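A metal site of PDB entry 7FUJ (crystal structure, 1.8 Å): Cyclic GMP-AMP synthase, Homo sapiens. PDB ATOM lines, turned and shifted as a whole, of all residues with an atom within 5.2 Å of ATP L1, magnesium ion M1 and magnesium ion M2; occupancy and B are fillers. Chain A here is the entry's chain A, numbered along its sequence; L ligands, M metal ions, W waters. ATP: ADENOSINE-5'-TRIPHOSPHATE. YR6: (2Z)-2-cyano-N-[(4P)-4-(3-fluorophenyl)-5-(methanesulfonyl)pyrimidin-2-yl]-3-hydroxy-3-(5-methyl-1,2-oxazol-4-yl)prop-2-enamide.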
ATOM      1  N   GLY A  52     -23.308  20.315  26.621  1.00  0.00           N
ATOM      2  CA  GLY A  52     -23.687  21.520  25.852  1.00  0.00           C
ATOM      3  C   GLY A  52     -23.886  22.731  26.736  1.00  0.00           C
ATOM      4  O   GLY A  52     -23.490  22.735  27.932  1.00  0.00           O
ATOM      5  N   SER A  53     -24.479  23.759  26.147  1.00  0.00           N
ATOM      6  CA  SER A  53     -24.336  25.154  26.593  1.00  0.00           C
ATOM      7  C   SER A  53     -25.065  25.365  27.921  1.00  0.00           C
ATOM      8  O   SER A  53     -24.582  26.162  28.729  1.00  0.00           O
ATOM      9  CB  SER A  53     -24.824  26.077  25.486  1.00  0.00           C
ATOM     10  OG  SER A  53     -26.215  25.919  25.229  1.00  0.00           O
ATOM     11  N   TYR A  54     -26.162  24.684  28.164  1.00  0.00           N
ATOM     12  CA  TYR A  54     -26.887  24.927  29.432  1.00  0.00           C
ATOM     13  C   TYR A  54     -25.997  24.492  30.609  1.00  0.00           C
ATOM     14  O   TYR A  54     -25.829  25.298  31.522  1.00  0.00           O
ATOM     15  CB  TYR A  54     -28.179  24.146  29.514  1.00  0.00           C
ATOM     16  CG  TYR A  54     -28.907  24.434  30.791  1.00  0.00           C
ATOM     17  CD1 TYR A  54     -29.705  25.546  30.918  1.00  0.00           C
ATOM     18  CD2 TYR A  54     -28.742  23.621  31.892  1.00  0.00           C
ATOM     19  CE1 TYR A  54     -30.372  25.817  32.086  1.00  0.00           C
ATOM     20  CE2 TYR A  54     -29.391  23.884  33.091  1.00  0.00           C
ATOM     21  CZ  TYR A  54     -30.228  24.981  33.178  1.00  0.00           C
ATOM     22  OH  TYR A  54     -30.911  25.193  34.346  1.00  0.00           O
ATOM     23  N   GLU A  56     -22.767  24.047  30.557  1.00  0.00           N
ATOM     24  CA  GLU A  56     -21.526  24.862  30.485  1.00  0.00           C
ATOM     25  C   GLU A  56     -21.765  26.307  30.935  1.00  0.00           C
ATOM     26  O   GLU A  56     -20.779  27.072  31.010  1.00  0.00           O
ATOM     27  CB  GLU A  56     -20.961  24.843  29.062  1.00  0.00           C
ATOM     28  CG  GLU A  56     -20.430  23.487  28.654  1.00  0.00           C
ATOM     29  CD  GLU A  56     -20.255  23.303  27.158  1.00  0.00           C
ATOM     30  OE1 GLU A  56     -20.801  24.133  26.382  1.00  0.00           O
ATOM     31  OE2 GLU A  56     -19.611  22.323  26.758  1.00  0.00           O
ATOM     32  N   LYS A  59     -25.343  28.981  27.697  1.00  0.00           N
ATOM     33  CA  LYS A  59     -26.672  29.166  27.037  1.00  0.00           C
ATOM     34  C   LYS A  59     -27.056  30.641  27.116  1.00  0.00           C
ATOM     35  O   LYS A  59     -26.828  31.267  28.172  1.00  0.00           O
ATOM     36  CB  LYS A  59     -27.783  28.296  27.652  1.00  0.00           C
ATOM     37  CG  LYS A  59     -29.128  28.345  26.944  1.00  0.00           C
ATOM     38  CD  LYS A  59     -29.193  27.415  25.773  1.00  0.00           C
ATOM     39  CE  LYS A  59     -30.469  27.542  24.975  1.00  0.00           C
ATOM     40  NZ  LYS A  59     -30.584  28.905  24.388  1.00  0.00           N
ATOM     41  N   GLU A  65     -33.160  24.912  25.338  1.00  0.00           N
ATOM     42  CA  GLU A  65     -32.467  23.833  24.579  1.00  0.00           C
ATOM     43  C   GLU A  65     -31.399  23.218  25.470  1.00  0.00           C
ATOM     44  O   GLU A  65     -30.456  23.949  25.865  1.00  0.00           O
ATOM     45  CB  GLU A  65     -31.869  24.358  23.261  1.00  0.00           C
ATOM     46  CG  GLU A  65     -31.605  23.239  22.237  1.00  0.00           C
ATOM     47  CD  GLU A  65     -30.212  22.628  22.202  1.00  0.00           C
ATOM     48  OE1 GLU A  65     -29.340  23.162  22.868  1.00  0.00           O
ATOM     49  OE2 GLU A  65     -30.031  21.558  21.577  1.00  0.00           O
ATOM     50  N   PHE A  66     -31.608  21.955  25.812  1.00  0.00           N
ATOM     51  CA  PHE A  66     -30.781  21.120  26.722  1.00  0.00           C
ATOM     52  C   PHE A  66     -30.196  19.968  25.913  1.00  0.00           C
ATOM     53  O   PHE A  66     -30.878  19.458  25.009  1.00  0.00           O
ATOM     54  CB  PHE A  66     -31.632  20.586  27.877  1.00  0.00           C
ATOM     55  CG  PHE A  66     -32.152  21.644  28.819  1.00  0.00           C
ATOM     56  CD1 PHE A  66     -33.187  22.499  28.425  1.00  0.00           C
ATOM     57  CD2 PHE A  66     -31.611  21.804  30.084  1.00  0.00           C
ATOM     58  CE1 PHE A  66     -33.649  23.487  29.278  1.00  0.00           C
ATOM     59  CE2 PHE A  66     -32.095  22.769  30.957  1.00  0.00           C
ATOM     60  CZ  PHE A  66     -33.102  23.611  30.554  1.00  0.00           C
ATOM     61  N   ASP A  67     -28.974  19.578  26.234  1.00  0.00           N
ATOM     62  CA  ASP A  67     -28.259  18.456  25.596  1.00  0.00           C
ATOM     63  C   ASP A  67     -27.909  17.418  26.672  1.00  0.00           C
ATOM     64  O   ASP A  67     -27.393  17.785  27.755  1.00  0.00           O
ATOM     65  CB  ASP A  67     -27.053  18.965  24.806  1.00  0.00           C
ATOM     66  CG  ASP A  67     -27.463  20.019  23.798  1.00  0.00           C
ATOM     67  OD1 ASP A  67     -28.090  19.625  22.744  1.00  0.00           O
ATOM     68  OD2 ASP A  67     -27.215  21.224  24.068  1.00  0.00           O
ATOM     69  N   ASP A 159     -32.141  17.537  23.274  1.00  0.00           N
ATOM     70  CA  ASP A 159     -31.392  16.651  22.353  1.00  0.00           C
ATOM     71  C   ASP A 159     -30.808  15.540  23.194  1.00  0.00           C
ATOM     72  O   ASP A 159     -30.054  15.844  24.131  1.00  0.00           O
ATOM     73  CB  ASP A 159     -30.263  17.358  21.581  1.00  0.00           C
ATOM     74  CG  ASP A 159     -30.761  18.385  20.572  1.00  0.00           C
ATOM     75  OD1 ASP A 159     -31.948  18.234  20.138  1.00  0.00           O
ATOM     76  OD2 ASP A 159     -29.988  19.342  20.252  1.00  0.00           O
ATOM     77  N   ARG A 216     -19.142   8.682  15.085  1.00  0.00           N
ATOM     78  CA  ARG A 216     -18.213   9.856  15.084  1.00  0.00           C
ATOM     79  C   ARG A 216     -17.723  10.105  16.508  1.00  0.00           C
ATOM     80  O   ARG A 216     -18.517   9.960  17.449  1.00  0.00           O
ATOM     81  CB  ARG A 216     -18.874  11.100  14.501  1.00  0.00           C
ATOM     82  CG  ARG A 216     -17.869  12.183  14.133  1.00  0.00           C
ATOM     83  CD  ARG A 216     -18.469  13.590  14.209  1.00  0.00           C
ATOM     84  NE  ARG A 216     -18.648  13.885  15.613  1.00  0.00           N
ATOM     85  CZ  ARG A 216     -19.694  14.486  16.173  1.00  0.00           C
ATOM     86  NH1 ARG A 216     -19.734  14.599  17.491  1.00  0.00           N
ATOM     87  NH2 ARG A 216     -20.703  14.944  15.464  1.00  0.00           N
ATOM     88  N   LEU A 217     -16.461  10.484  16.651  1.00  0.00           N
ATOM     89  CA  LEU A 217     -15.918  10.774  18.005  1.00  0.00           C
ATOM     90  C   LEU A 217     -16.712  11.942  18.631  1.00  0.00           C
ATOM     91  O   LEU A 217     -17.150  12.868  17.865  1.00  0.00           O
ATOM     92  CB  LEU A 217     -14.437  11.120  17.911  1.00  0.00           C
ATOM     93  CG  LEU A 217     -13.501  10.010  17.476  1.00  0.00           C
ATOM     94  CD1 LEU A 217     -12.076  10.502  17.409  1.00  0.00           C
ATOM     95  CD2 LEU A 217     -13.604   8.835  18.407  1.00  0.00           C
ATOM     96  N   SER A 220     -17.655  15.994  24.104  1.00  0.00           N
ATOM     97  CA  SER A 220     -18.582  16.915  24.812  1.00  0.00           C
ATOM     98  C   SER A 220     -18.272  16.960  26.316  1.00  0.00           C
ATOM     99  O   SER A 220     -18.398  18.027  26.902  1.00  0.00           O
ATOM    100  CB  SER A 220     -19.995  16.537  24.567  1.00  0.00           C
ATOM    101  OG  SER A 220     -20.248  16.577  23.193  1.00  0.00           O
ATOM    102  N   GLU A 223     -15.115  19.145  26.723  1.00  0.00           N
ATOM    103  CA  GLU A 223     -15.500  20.553  26.463  1.00  0.00           C
ATOM    104  C   GLU A 223     -16.195  21.133  27.697  1.00  0.00           C
ATOM    105  O   GLU A 223     -15.879  22.275  28.078  1.00  0.00           O
ATOM    106  CB  GLU A 223     -16.424  20.642  25.249  1.00  0.00           C
ATOM    107  CG  GLU A 223     -15.772  20.136  24.003  1.00  0.00           C
ATOM    108  CD  GLU A 223     -16.712  19.969  22.822  1.00  0.00           C
ATOM    109  OE1 GLU A 223     -17.873  20.465  22.911  1.00  0.00           O
ATOM    110  OE2 GLU A 223     -16.265  19.359  21.805  1.00  0.00           O
ATOM    111  N   LYS A 254     -21.649  33.569  20.274  1.00  0.00           N
ATOM    112  CA  LYS A 254     -22.868  32.765  20.047  1.00  0.00           C
ATOM    113  C   LYS A 254     -24.008  33.676  19.581  1.00  0.00           C
ATOM    114  O   LYS A 254     -24.727  33.303  18.646  1.00  0.00           O
ATOM    115  CB  LYS A 254     -23.250  32.011  21.320  1.00  0.00           C
ATOM    116  CG  LYS A 254     -22.303  30.857  21.656  1.00  0.00           C
ATOM    117  CD  LYS A 254     -22.512  30.223  23.000  1.00  0.00           C
ATOM    118  CE  LYS A 254     -23.877  29.552  23.180  1.00  0.00           C
ATOM    119  NZ  LYS A 254     -24.108  28.478  22.199  1.00  0.00           N
ATOM    120  N   GLU A 258     -26.209  33.590  16.223  1.00  0.00           N
ATOM    121  CA  GLU A 258     -27.682  33.361  16.355  1.00  0.00           C
ATOM    122  C   GLU A 258     -28.430  34.501  15.633  1.00  0.00           C
ATOM    123  O   GLU A 258     -29.379  34.209  14.883  1.00  0.00           O
ATOM    124  CB  GLU A 258     -28.124  33.215  17.821  1.00  0.00           C
ATOM    125  CG  GLU A 258     -27.909  31.808  18.400  1.00  0.00           C
ATOM    126  CD  GLU A 258     -28.469  31.616  19.815  1.00  0.00           C
ATOM    127  OE1 GLU A 258     -29.480  32.310  20.144  1.00  0.00           O
ATOM    128  OE2 GLU A 258     -27.918  30.772  20.602  1.00  0.00           O
ATOM    129  N   SER A 275     -23.376  26.828  16.196  1.00  0.00           N
ATOM    130  CA  SER A 275     -22.753  27.345  17.439  1.00  0.00           C
ATOM    131  C   SER A 275     -21.455  26.581  17.684  1.00  0.00           C
ATOM    132  O   SER A 275     -20.567  27.173  18.280  1.00  0.00           O
ATOM    133  CB  SER A 275     -23.709  27.263  18.627  1.00  0.00           C
ATOM    134  OG  SER A 275     -23.958  25.909  18.999  1.00  0.00           O
ATOM    135  N   TYR A 276     -21.310  25.342  17.230  1.00  0.00           N
ATOM    136  CA  TYR A 276     -20.086  24.534  17.456  1.00  0.00           C
ATOM    137  C   TYR A 276     -18.904  25.164  16.704  1.00  0.00           C
ATOM    138  O   TYR A 276     -17.779  25.004  17.161  1.00  0.00           O
ATOM    139  CB  TYR A 276     -20.240  23.068  17.050  1.00  0.00           C
ATOM    140  CG  TYR A 276     -19.148  22.200  17.604  1.00  0.00           C
ATOM    141  CD1 TYR A 276     -18.937  22.091  18.978  1.00  0.00           C
ATOM    142  CD2 TYR A 276     -18.245  21.563  16.773  1.00  0.00           C
ATOM    143  CE1 TYR A 276     -17.911  21.319  19.491  1.00  0.00           C
ATOM    144  CE2 TYR A 276     -17.219  20.790  17.276  1.00  0.00           C
ATOM    145  CZ  TYR A 276     -17.065  20.652  18.629  1.00  0.00           C
ATOM    146  OH  TYR A 276     -16.026  19.906  19.122  1.00  0.00           O
ATOM    147  N   LYS A 279     -17.854  27.861  19.068  1.00  0.00           N
ATOM    148  CA  LYS A 279     -17.305  27.229  20.313  1.00  0.00           C
ATOM    149  C   LYS A 279     -15.879  26.755  20.027  1.00  0.00           C
ATOM    150  O   LYS A 279     -14.956  27.016  20.857  1.00  0.00           O
ATOM    151  CB  LYS A 279     -18.167  26.050  20.775  1.00  0.00           C
ATOM    152  CG  LYS A 279     -17.822  25.531  22.165  1.00  0.00           C
ATOM    153  CD  LYS A 279     -18.505  24.183  22.421  1.00  0.00           C
ATOM    154  CE  LYS A 279     -18.445  23.737  23.857  1.00  0.00           C
ATOM    155  NZ  LYS A 279     -19.154  22.478  24.112  1.00  0.00           N
ATOM    156  N   ASN A 322     -11.153  20.958  14.234  1.00  0.00           N
ATOM    157  CA  ASN A 322     -11.723  20.343  15.454  1.00  0.00           C
ATOM    158  C   ASN A 322     -10.654  20.452  16.547  1.00  0.00           C
ATOM    159  O   ASN A 322      -9.457  20.179  16.266  1.00  0.00           O
ATOM    160  CB  ASN A 322     -12.231  18.948  15.182  1.00  0.00           C
ATOM    161  CG  ASN A 322     -12.776  18.267  16.403  1.00  0.00           C
ATOM    162  OD1 ASN A 322     -12.053  18.015  17.375  1.00  0.00           O
ATOM    163  ND2 ASN A 322     -14.055  17.928  16.350  1.00  0.00           N
ATOM    164  N   LEU A 330     -13.519  21.642  10.004  1.00  0.00           N
ATOM    165  CA  LEU A 330     -14.975  21.941  10.072  1.00  0.00           C
ATOM    166  C   LEU A 330     -15.390  22.854   8.916  1.00  0.00           C
ATOM    167  O   LEU A 330     -16.586  22.861   8.610  1.00  0.00           O
ATOM    168  CB  LEU A 330     -15.343  22.594  11.400  1.00  0.00           C
ATOM    169  CG  LEU A 330     -15.067  21.766  12.653  1.00  0.00           C
ATOM    170  CD1 LEU A 330     -15.281  22.591  13.911  1.00  0.00           C
ATOM    171  CD2 LEU A 330     -15.950  20.551  12.694  1.00  0.00           C
HETATM  172  PG  ATP L   1     -26.338  25.967  21.807  1.00  0.00           P
HETATM  173  O1G ATP L   1     -27.264  24.783  21.988  1.00  0.00           O
HETATM  174  O2G ATP L   1     -26.248  26.456  20.382  1.00  0.00           O
HETATM  175  O3G ATP L   1     -26.520  27.050  22.822  1.00  0.00           O
HETATM  176  PB  ATP L   1     -24.393  23.843  22.317  1.00  0.00           P
HETATM  177  O1B ATP L   1     -22.936  23.708  22.567  1.00  0.00           O
HETATM  178  O2B ATP L   1     -25.354  23.303  23.360  1.00  0.00           O
HETATM  179  O3B ATP L   1     -24.825  25.371  22.124  1.00  0.00           O
HETATM  180  PA  ATP L   1     -25.602  21.985  20.341  1.00  0.00           P
HETATM  181  O1A ATP L   1     -25.806  22.156  18.876  1.00  0.00           O
HETATM  182  O2A ATP L   1     -26.795  21.854  21.257  1.00  0.00           O
HETATM  183  O3A ATP L   1     -24.802  23.262  20.887  1.00  0.00           O
HETATM  184  O5' ATP L   1     -24.590  20.801  20.568  1.00  0.00           O
HETATM  185  C5' ATP L   1     -24.467  20.150  21.867  1.00  0.00           C
HETATM  186  C4' ATP L   1     -23.055  19.663  22.021  1.00  0.00           C
HETATM  187  O4' ATP L   1     -22.799  18.624  21.046  1.00  0.00           O
HETATM  188  C3' ATP L   1     -21.946  20.689  21.774  1.00  0.00           C
HETATM  189  O3' ATP L   1     -21.585  21.519  22.870  1.00  0.00           O
HETATM  190  C2' ATP L   1     -20.768  19.778  21.380  1.00  0.00           C
HETATM  191  O2' ATP L   1     -20.114  19.229  22.485  1.00  0.00           O
HETATM  192  C1' ATP L   1     -21.467  18.695  20.563  1.00  0.00           C
HETATM  193  N9  ATP L   1     -21.465  18.983  19.129  1.00  0.00           N
HETATM  194  C8  ATP L   1     -22.370  19.722  18.379  1.00  0.00           C
HETATM  195  N7  ATP L   1     -22.023  19.834  17.122  1.00  0.00           N
HETATM  196  C5  ATP L   1     -20.839  19.097  17.016  1.00  0.00           C
HETATM  197  C6  ATP L   1     -19.997  18.804  15.920  1.00  0.00           C
HETATM  198  N6  ATP L   1     -20.210  19.232  14.673  1.00  0.00           N
HETATM  199  N1  ATP L   1     -18.923  18.030  16.163  1.00  0.00           N
HETATM  200  C2  ATP L   1     -18.714  17.593  17.411  1.00  0.00           C
HETATM  201  N3  ATP L   1     -19.419  17.825  18.520  1.00  0.00           N
HETATM  202  C4  ATP L   1     -20.491  18.576  18.237  1.00  0.00           C
HETATM  203  C10 YR6 L   2     -24.277  18.403  13.838  1.00  0.00           C
HETATM  204  O14 YR6 L   2     -23.128  18.404  11.492  1.00  0.00           O
HETATM  205  C15 YR6 L   2     -25.237  18.749  14.831  1.00  0.00           C
HETATM  206  C16 YR6 L   2     -26.372  19.681  14.655  1.00  0.00           C
HETATM  207  C17 YR6 L   2     -27.379  19.425  13.715  1.00  0.00           C
HETATM  208  C18 YR6 L   2     -28.445  20.294  13.561  1.00  0.00           C
HETATM  209  C19 YR6 L   2     -28.576  21.408  14.377  1.00  0.00           C
HETATM  210  C20 YR6 L   2     -27.603  21.614  15.338  1.00  0.00           C
HETATM  211  C21 YR6 L   2     -26.504  20.796  15.491  1.00  0.00           C
HETATM  212  C24 YR6 L   2     -24.516  16.222  20.350  1.00  0.00           C
HETATM  213  C26 YR6 L   2     -24.681  16.007  21.760  1.00  0.00           C
HETATM  214  C27 YR6 L   2     -25.819  15.917  22.516  1.00  0.00           C
HETATM  215  N1  YR6 L   2     -21.533  14.477  20.699  1.00  0.00           N
HETATM  216  C2  YR6 L   2     -22.386  15.074  20.231  1.00  0.00           C
HETATM  217  C3  YR6 L   2     -23.427  15.809  19.609  1.00  0.00           C
HETATM  218  C4  YR6 L   2     -23.190  16.134  18.208  1.00  0.00           C
HETATM  219  O5  YR6 L   2     -22.175  15.711  17.636  1.00  0.00           O
HETATM  220  N6  YR6 L   2     -24.174  16.799  17.567  1.00  0.00           N
HETATM  221  C7  YR6 L   2     -24.210  17.280  16.281  1.00  0.00           C
HETATM  222  N8  YR6 L   2     -23.235  16.928  15.438  1.00  0.00           N
HETATM  223  C9  YR6 L   2     -23.310  17.470  14.221  1.00  0.00           C
HETATM  224  S11 YR6 L   2     -24.183  19.086  12.191  1.00  0.00           S
HETATM  225  C12 YR6 L   2     -25.689  18.746  11.384  1.00  0.00           C
HETATM  226  O13 YR6 L   2     -24.065  20.512  12.347  1.00  0.00           O
HETATM  227  F22 YR6 L   2     -27.719  22.689  16.154  1.00  0.00           F
HETATM  228  N23 YR6 L   2     -25.183  18.183  16.058  1.00  0.00           N
HETATM  229  O25 YR6 L   2     -25.480  16.934  19.809  1.00  0.00           O
HETATM  230  O28 YR6 L   2     -25.487  15.830  23.812  1.00  0.00           O
HETATM  231  N29 YR6 L   2     -24.086  15.884  23.930  1.00  0.00           N
HETATM  232  C30 YR6 L   2     -23.647  16.033  22.714  1.00  0.00           C
HETATM  233  C31 YR6 L   2     -27.259  15.868  22.207  1.00  0.00           C
HETATM  234 MG    MG M   1     -28.406  20.436  20.901  1.00  0.00          MG
HETATM  235 MG    MG M   2     -27.301  22.976  23.058  1.00  0.00          MG
HETATM  236  O   HOH W   1     -16.472  17.772  14.769  1.00  0.00           O
HETATM  237  O   HOH W   2     -27.831  29.532  23.327  1.00  0.00           O
HETATM  238  O   HOH W   3     -27.770  23.819  24.902  1.00  0.00           O
HETATM  239  O   HOH W   4     -27.315  24.940  18.395  1.00  0.00           O
HETATM  240  O   HOH W   5     -21.754  24.987  20.289  1.00  0.00           O
HETATM  241  O   HOH W   6     -23.104  21.435  15.240  1.00  0.00           O
HETATM  242  O   HOH W   7     -24.000  23.488  17.315  1.00  0.00           O
HETATM  243  O   HOH W   8     -21.551  25.530  24.216  1.00  0.00           O
HETATM  244  O   HOH W   9     -27.115  19.164  19.872  1.00  0.00           O
HETATM  245  O   HOH W  10     -25.595  29.503  20.107  1.00  0.00           O
HETATM  246  O   HOH W  11     -28.664  21.428  19.106  1.00  0.00           O
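N of Asp 159 sits at hydrogen-bond distance from O of Phe 66, 2.9 Å away.
NZ of Lys 279 is in salt-bridge range of OE1 of Glu 223 (2.7 Å).
The side-chain hydroxyl (OH) of Tyr 276 is in hydrogen-bond range of the side-chain carboxylate (OE2) of Glu 223, 2.7 Å away.
O of Ser 53 lies within hydrogen-bond range of N of Lys 59, 3.1 Å away.
OE2 of Glu 56 is in salt-bridge range of NZ of Lys 279, 2.7 Å away.
O4' of ATP L1 lies close to O25 of YR6 L2, 3.4 Å away.
The side-chain carboxylate (OE1) of Glu 223 lies within hydrogen-bond range of an oxygen (O2') of ATP L1 (2.6 Å).
The backbone NH (N) of Ser 53 sits close to an oxygen (O2B) of ATP L1, 3.0 Å away.
OG of Ser 53 sits at hydrogen-bond distance from O3G of ATP L1, 2.7 Å away.
OG of Ser 275 lies within hydrogen-bond range of O2G of ATP L1 (2.7 Å).
The side-chain hydroxyl of Ser 220 lies within hydrogen-bond range of an oxygen (O2') of ATP L1 (2.7 Å).
The side-chain amino group (NZ) of Lys 254 lies within salt-bridge range of an oxygen (O3G) of ATP L1.
An oxygen (O3') of ATP L1 is in hydrogen-bond range of the side-chain amino group (NZ) of Lys 279, at 2.9 Å.
NH1 of Arg 216 sits close to N3 of ATP L1 (3.4 Å).
The guanidinium group of Arg 216 is in hydrogen-bond range of an oxygen (O5) of YR6 L2 (2.7 Å).
Water W9 bridges an oxygen (O25) of YR6 L2 (2.8 Å) and an oxygen (O5') of ATP L1 (3.1 Å).
Water W3 bridges OG of Ser 53 (2.6 Å) and O of Glu 65 (2.9 Å).
Water W7 lies within hydrogen-bond range of an oxygen (O1A) of ATP L1 (2.7 Å), the side-chain hydroxyl of Ser 275 (2.9 Å) and the backbone NH of Tyr 276 (3.3 Å).
Water W1 lies within hydrogen-bond range of N1 of ATP L1 and ND2 of Asn 322.
Water W5 lies within hydrogen-bond range of the side-chain hydroxyl (OG) of Ser 275, an oxygen (O1B) of ATP L1 and the backbone NH (N) of Tyr 276.
Water W10 lies within hydrogen-bond range of the side-chain carboxylate (OE2) of Glu 258, the side-chain amino group (NZ) of Lys 254 and an oxygen (O2G) of ATP L1.
Three residues have an atom within 4 Å of magnesium ion M1: Glu 65, Asp 67 and Asp 159.
Merely in contact with magnesium ion M2: Ser 53 (3.8 Å).
The nearest printed residue that does not touch magnesium ion M2 is Gly 52 (4.8 Å).
Magnesium ion M2 is bound by an oxygen (O2B) of ATP L1 (2.0 Å), the side-chain carboxylate (OD2) of Asp 67 (2.0 Å), the side-chain carboxylate (OE1) of Glu 65 (2.1 Å), water W3 (2.1 Å), an oxygen (O1G) of ATP L1 (2.1 Å) and an oxygen (O2A) of ATP L1 (2.2 Å).
Residues that only touch ATP L1: Tyr 276 (3.4 Å), Gly 52 (3.5 Å) and Lys 59 (3.998 Å).
Hydrophobic or aromatic side chains that line ATP L1: Tyr 276.
Of the 20 residues printed, 12 come within 4 Å of ATP L1.
Magnesium ion M1 is bound by OD2 of Asp 159 (2.0 Å), OD1 of Asp 67 (2.0 Å), water W11 (2.1 Å), water W9 (2.1 Å), OE2 of Glu 65 (2.1 Å) and O2A of ATP L1 (2.2 Å).
Magnesium ion M1 has six donor atoms within binding distance.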
